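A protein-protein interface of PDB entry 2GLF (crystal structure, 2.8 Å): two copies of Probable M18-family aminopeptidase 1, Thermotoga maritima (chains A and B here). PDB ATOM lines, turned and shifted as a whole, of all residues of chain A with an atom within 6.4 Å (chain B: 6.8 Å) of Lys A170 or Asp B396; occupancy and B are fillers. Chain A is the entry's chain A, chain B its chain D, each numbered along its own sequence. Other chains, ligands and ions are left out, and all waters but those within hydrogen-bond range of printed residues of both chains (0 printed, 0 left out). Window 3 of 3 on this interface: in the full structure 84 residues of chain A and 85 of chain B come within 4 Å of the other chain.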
ATOM      1  N   LEU A 164     -26.848 -12.203  11.390  1.00  0.00           N
ATOM      2  CA  LEU A 164     -25.545 -12.716  10.960  1.00  0.00           C
ATOM      3  C   LEU A 164     -24.816 -11.679  10.125  1.00  0.00           C
ATOM      4  O   LEU A 164     -25.417 -11.070   9.240  1.00  0.00           O
ATOM      5  CB  LEU A 164     -25.733 -13.990  10.136  1.00  0.00           C
ATOM      6  CG  LEU A 164     -24.501 -14.753   9.652  1.00  0.00           C
ATOM      7  CD1 LEU A 164     -23.635 -15.146  10.823  1.00  0.00           C
ATOM      8  CD2 LEU A 164     -24.942 -15.999   8.899  1.00  0.00           C
ATOM      9  N   PRO A 166     -22.837  -9.847   7.283  1.00  0.00           N
ATOM     10  CA  PRO A 166     -22.869 -10.086   5.840  1.00  0.00           C
ATOM     11  C   PRO A 166     -21.709 -10.886   5.254  1.00  0.00           C
ATOM     12  O   PRO A 166     -21.892 -11.647   4.305  1.00  0.00           O
ATOM     13  CB  PRO A 166     -22.962  -8.675   5.264  1.00  0.00           C
ATOM     14  CG  PRO A 166     -22.238  -7.840   6.277  1.00  0.00           C
ATOM     15  CD  PRO A 166     -22.757  -8.402   7.576  1.00  0.00           C
ATOM     16  N   HIS A 167     -20.524 -10.727   5.833  1.00  0.00           N
ATOM     17  CA  HIS A 167     -19.329 -11.409   5.351  1.00  0.00           C
ATOM     18  C   HIS A 167     -19.435 -12.928   5.299  1.00  0.00           C
ATOM     19  O   HIS A 167     -18.822 -13.572   4.448  1.00  0.00           O
ATOM     20  CB  HIS A 167     -18.132 -11.055   6.225  1.00  0.00           C
ATOM     21  CG  HIS A 167     -18.052  -9.609   6.587  1.00  0.00           C
ATOM     22  ND1 HIS A 167     -16.853  -8.940   6.690  1.00  0.00           N
ATOM     23  CD2 HIS A 167     -19.017  -8.706   6.879  1.00  0.00           C
ATOM     24  CE1 HIS A 167     -17.083  -7.683   7.026  1.00  0.00           C
ATOM     25  NE2 HIS A 167     -18.389  -7.517   7.147  1.00  0.00           N
ATOM     26  N   LEU A 168     -20.197 -13.503   6.217  1.00  0.00           N
ATOM     27  CA  LEU A 168     -20.337 -14.948   6.274  1.00  0.00           C
ATOM     28  C   LEU A 168     -21.706 -15.430   5.831  1.00  0.00           C
ATOM     29  O   LEU A 168     -21.976 -16.632   5.853  1.00  0.00           O
ATOM     30  CB  LEU A 168     -20.032 -15.437   7.694  1.00  0.00           C
ATOM     31  CG  LEU A 168     -18.600 -15.877   8.018  1.00  0.00           C
ATOM     32  CD1 LEU A 168     -17.588 -15.027   7.294  1.00  0.00           C
ATOM     33  CD2 LEU A 168     -18.385 -15.816   9.513  1.00  0.00           C
ATOM     34  N   ASP A 169     -22.563 -14.495   5.429  1.00  0.00           N
ATOM     35  CA  ASP A 169     -23.911 -14.825   4.965  1.00  0.00           C
ATOM     36  C   ASP A 169     -23.803 -15.043   3.460  1.00  0.00           C
ATOM     37  O   ASP A 169     -23.907 -14.097   2.678  1.00  0.00           O
ATOM     38  CB  ASP A 169     -24.868 -13.667   5.272  1.00  0.00           C
ATOM     39  CG  ASP A 169     -26.323 -14.095   5.284  1.00  0.00           C
ATOM     40  OD1 ASP A 169     -26.813 -14.572   4.242  1.00  0.00           O
ATOM     41  OD2 ASP A 169     -26.975 -13.949   6.340  1.00  0.00           O
ATOM     42  N   LYS A 170     -23.600 -16.297   3.066  1.00  0.00           N
ATOM     43  CA  LYS A 170     -23.414 -16.655   1.664  1.00  0.00           C
ATOM     44  C   LYS A 170     -24.645 -17.144   0.898  1.00  0.00           C
ATOM     45  O   LYS A 170     -24.646 -17.147  -0.334  1.00  0.00           O
ATOM     46  CB  LYS A 170     -22.293 -17.696   1.572  1.00  0.00           C
ATOM     47  CG  LYS A 170     -21.949 -18.164   0.169  1.00  0.00           C
ATOM     48  CD  LYS A 170     -20.641 -18.954   0.143  1.00  0.00           C
ATOM     49  CE  LYS A 170     -20.689 -20.201   1.019  1.00  0.00           C
ATOM     50  NZ  LYS A 170     -20.759 -19.889   2.473  1.00  0.00           N
ATOM     51  N   GLU A 171     -25.687 -17.547   1.617  1.00  0.00           N
ATOM     52  CA  GLU A 171     -26.900 -18.045   0.978  1.00  0.00           C
ATOM     53  C   GLU A 171     -27.832 -16.941   0.501  1.00  0.00           C
ATOM     54  O   GLU A 171     -28.494 -16.282   1.307  1.00  0.00           O
ATOM     55  CB  GLU A 171     -27.655 -18.974   1.931  1.00  0.00           C
ATOM     56  CG  GLU A 171     -27.344 -20.452   1.738  1.00  0.00           C
ATOM     57  CD  GLU A 171     -25.855 -20.743   1.685  1.00  0.00           C
ATOM     58  OE1 GLU A 171     -25.144 -20.394   2.651  1.00  0.00           O
ATOM     59  OE2 GLU A 171     -25.397 -21.324   0.678  1.00  0.00           O
ATOM     60  N   ASP A 172     -27.885 -16.753  -0.817  1.00  0.00           N
ATOM     61  CA  ASP A 172     -28.739 -15.738  -1.429  1.00  0.00           C
ATOM     62  C   ASP A 172     -30.150 -16.291  -1.628  1.00  0.00           C
ATOM     63  O   ASP A 172     -30.662 -16.314  -2.747  1.00  0.00           O
ATOM     64  CB  ASP A 172     -28.157 -15.314  -2.777  1.00  0.00           C
ATOM     65  CG  ASP A 172     -28.868 -14.116  -3.365  1.00  0.00           C
ATOM     66  OD1 ASP A 172     -28.788 -13.022  -2.766  1.00  0.00           O
ATOM     67  OD2 ASP A 172     -29.509 -14.267  -4.425  1.00  0.00           O
ATOM     68  N   ALA A 173     -30.771 -16.732  -0.536  1.00  0.00           N
ATOM     69  CA  ALA A 173     -32.119 -17.306  -0.573  1.00  0.00           C
ATOM     70  C   ALA A 173     -33.226 -16.261  -0.694  1.00  0.00           C
ATOM     71  O   ALA A 173     -32.971 -15.061  -0.585  1.00  0.00           O
ATOM     72  CB  ALA A 173     -32.350 -18.157   0.671  1.00  0.00           C
ATOM     73  N   VAL B 338     -21.642 -21.486  10.552  1.00  0.00           N
ATOM     74  CA  VAL B 338     -20.755 -20.719   9.683  1.00  0.00           C
ATOM     75  C   VAL B 338     -19.307 -20.670  10.197  1.00  0.00           C
ATOM     76  O   VAL B 338     -18.391 -20.262   9.476  1.00  0.00           O
ATOM     77  CB  VAL B 338     -21.281 -19.281   9.544  1.00  0.00           C
ATOM     78  CG1 VAL B 338     -20.457 -18.532   8.552  1.00  0.00           C
ATOM     79  CG2 VAL B 338     -22.725 -19.302   9.112  1.00  0.00           C
ATOM     80  N   ALA B 359      -9.757 -14.575   1.925  1.00  0.00           N
ATOM     81  CA  ALA B 359     -10.785 -15.473   1.412  1.00  0.00           C
ATOM     82  C   ALA B 359     -10.229 -16.567   0.513  1.00  0.00           C
ATOM     83  O   ALA B 359      -9.120 -16.454  -0.003  1.00  0.00           O
ATOM     84  CB  ALA B 359     -11.828 -14.669   0.641  1.00  0.00           C
ATOM     85  N   ARG B 360     -11.010 -17.628   0.339  1.00  0.00           N
ATOM     86  CA  ARG B 360     -10.643 -18.734  -0.532  1.00  0.00           C
ATOM     87  C   ARG B 360      -9.196 -19.213  -0.413  1.00  0.00           C
ATOM     88  O   ARG B 360      -8.493 -19.324  -1.420  1.00  0.00           O
ATOM     89  CB  ARG B 360     -10.913 -18.338  -1.988  1.00  0.00           C
ATOM     90  CG  ARG B 360     -12.344 -17.914  -2.281  1.00  0.00           C
ATOM     91  CD  ARG B 360     -13.283 -19.089  -2.168  1.00  0.00           C
ATOM     92  NE  ARG B 360     -12.779 -20.222  -2.934  1.00  0.00           N
ATOM     93  CZ  ARG B 360     -13.382 -21.403  -3.010  1.00  0.00           C
ATOM     94  NH1 ARG B 360     -14.520 -21.613  -2.366  1.00  0.00           N
ATOM     95  NH2 ARG B 360     -12.840 -22.376  -3.725  1.00  0.00           N
ATOM     96  N   GLY B 361      -8.737 -19.506   0.794  1.00  0.00           N
ATOM     97  CA  GLY B 361      -7.366 -19.977   0.926  1.00  0.00           C
ATOM     98  C   GLY B 361      -6.339 -18.882   1.152  1.00  0.00           C
ATOM     99  O   GLY B 361      -5.270 -18.877   0.535  1.00  0.00           O
ATOM    100  N   GLY B 393     -14.618 -17.642  10.100  1.00  0.00           N
ATOM    101  CA  GLY B 393     -15.549 -18.593   9.503  1.00  0.00           C
ATOM    102  C   GLY B 393     -14.905 -19.861   8.959  1.00  0.00           C
ATOM    103  O   GLY B 393     -13.681 -19.922   8.807  1.00  0.00           O
ATOM    104  N   LYS B 394     -15.713 -20.880   8.663  1.00  0.00           N
ATOM    105  CA  LYS B 394     -15.171 -22.127   8.122  1.00  0.00           C
ATOM    106  C   LYS B 394     -14.311 -21.744   6.922  1.00  0.00           C
ATOM    107  O   LYS B 394     -14.470 -20.653   6.381  1.00  0.00           O
ATOM    108  CB  LYS B 394     -16.288 -23.074   7.672  1.00  0.00           C
ATOM    109  CG  LYS B 394     -17.172 -23.674   8.769  1.00  0.00           C
ATOM    110  CD  LYS B 394     -17.938 -24.864   8.193  1.00  0.00           C
ATOM    111  CE  LYS B 394     -19.178 -25.266   8.989  1.00  0.00           C
ATOM    112  NZ  LYS B 394     -18.907 -25.845  10.332  1.00  0.00           N
ATOM    113  N   VAL B 395     -13.422 -22.635   6.495  1.00  0.00           N
ATOM    114  CA  VAL B 395     -12.520 -22.343   5.382  1.00  0.00           C
ATOM    115  C   VAL B 395     -13.043 -21.483   4.230  1.00  0.00           C
ATOM    116  O   VAL B 395     -12.460 -20.430   3.947  1.00  0.00           O
ATOM    117  CB  VAL B 395     -11.892 -23.641   4.810  1.00  0.00           C
ATOM    118  CG1 VAL B 395     -11.317 -23.398   3.418  1.00  0.00           C
ATOM    119  CG2 VAL B 395     -10.765 -24.090   5.714  1.00  0.00           C
ATOM    120  N   ASP B 396     -14.115 -21.890   3.557  1.00  0.00           N
ATOM    121  CA  ASP B 396     -14.599 -21.065   2.451  1.00  0.00           C
ATOM    122  C   ASP B 396     -15.919 -20.306   2.656  1.00  0.00           C
ATOM    123  O   ASP B 396     -16.783 -20.300   1.776  1.00  0.00           O
ATOM    124  CB  ASP B 396     -14.664 -21.890   1.156  1.00  0.00           C
ATOM    125  CG  ASP B 396     -13.303 -22.003   0.457  1.00  0.00           C
ATOM    126  OD1 ASP B 396     -12.613 -20.965   0.329  1.00  0.00           O
ATOM    127  OD2 ASP B 396     -12.928 -23.121   0.020  1.00  0.00           O
ATOM    128  N   GLN B 397     -16.065 -19.655   3.811  1.00  0.00           N
ATOM    129  CA  GLN B 397     -17.263 -18.865   4.110  1.00  0.00           C
ATOM    130  C   GLN B 397     -17.171 -17.454   3.508  1.00  0.00           C
ATOM    131  O   GLN B 397     -18.190 -16.858   3.184  1.00  0.00           O
ATOM    132  CB  GLN B 397     -17.483 -18.750   5.622  1.00  0.00           C
ATOM    133  CG  GLN B 397     -18.204 -19.926   6.252  1.00  0.00           C
ATOM    134  CD  GLN B 397     -19.614 -20.105   5.718  1.00  0.00           C
ATOM    135  OE1 GLN B 397     -20.449 -19.203   5.811  1.00  0.00           O
ATOM    136  NE2 GLN B 397     -19.884 -21.277   5.157  1.00  0.00           N
ATOM    137  N   GLY B 398     -15.957 -16.917   3.380  1.00  0.00           N
ATOM    138  CA  GLY B 398     -15.794 -15.598   2.788  1.00  0.00           C
ATOM    139  C   GLY B 398     -15.265 -14.476   3.666  1.00  0.00           C
ATOM    140  O   GLY B 398     -14.358 -14.678   4.473  1.00  0.00           O
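The backbone carbonyl oxygen (O) of Leu A168 sits close to the side-chain amide oxygen (OE1) of Gln B397, at 3.0 Å.
NZ of Lys A170 lies close to NE2 of Gln B397 (3.1 Å).
The backbone carbonyl oxygen of Val B338 sits at hydrogen-bond distance from the backbone NH of Lys B394, at 2.9 Å.
NH1 of Arg B360 lies within salt-bridge range of OD2 of Asp B396 (3.2 Å).
Among the printed residues, pairs that only touch across the chains: Leu A168 with Val B338 (3.2 Å), His A167 with Gln B397 (3.6 Å), His A167 with Gly B398 (3.8 Å), Leu A168 with Gly B393 (3.97 Å), Lys A170 with Asp B396 (3.98 Å) and Leu A164 with Val B338 (3.98 Å).
Of chain B, only Asp B396 (3.98 Å) and Gln B397 (3.1 Å) come within 4 Å of Lys A170.
Asp B396 touches just one residue of chain A: Lys A170.
Of the printed residues of chain B, Leu A164 touches Val B338.
Of the printed residues of chain A, Gln B397 touches His A167 (3.6 Å), Leu A168 (3.0 Å) and Lys A170 (3.1 Å).
Gly B361 touches none of the printed residues of chain A.
The nearest residue of chain B that does not touch Lys A170 is Gly B398 (5.7 Å).
The nearest printed residue of chain A that does not touch Asp B396 is Leu A168 (7.2 Å).
The nearest printed residue of chain A that does not touch Gly B398 is Leu A168 (4.3 Å).
Of the 9 printed residues of chain A, 4 touch a printed residue of chain B.
Printed residues of chain A that touch a printed residue of chain B: Leu A164, His A167, Leu A168 and Lys A170.
Hydrophobic or aromatic side chains of chain A within 4 Å of the printed part of chain B: Leu A164 and Leu A168.
Of the 10 printed residues of chain B, 5 touch a printed residue of chain A.
Printed residues of chain B that touch a printed residue of chain A: Val B338, Gly B393, Asp B396, Gln B397 and Gly B398.
Hydrophobic or aromatic side chains of chain B within 4 Å of the printed part of chain A: Val B338.
No position is printed for both chains.
Of the 8 pairs that touch across the chains among the printed residues, none has its exchanged pair printed and touching as well.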
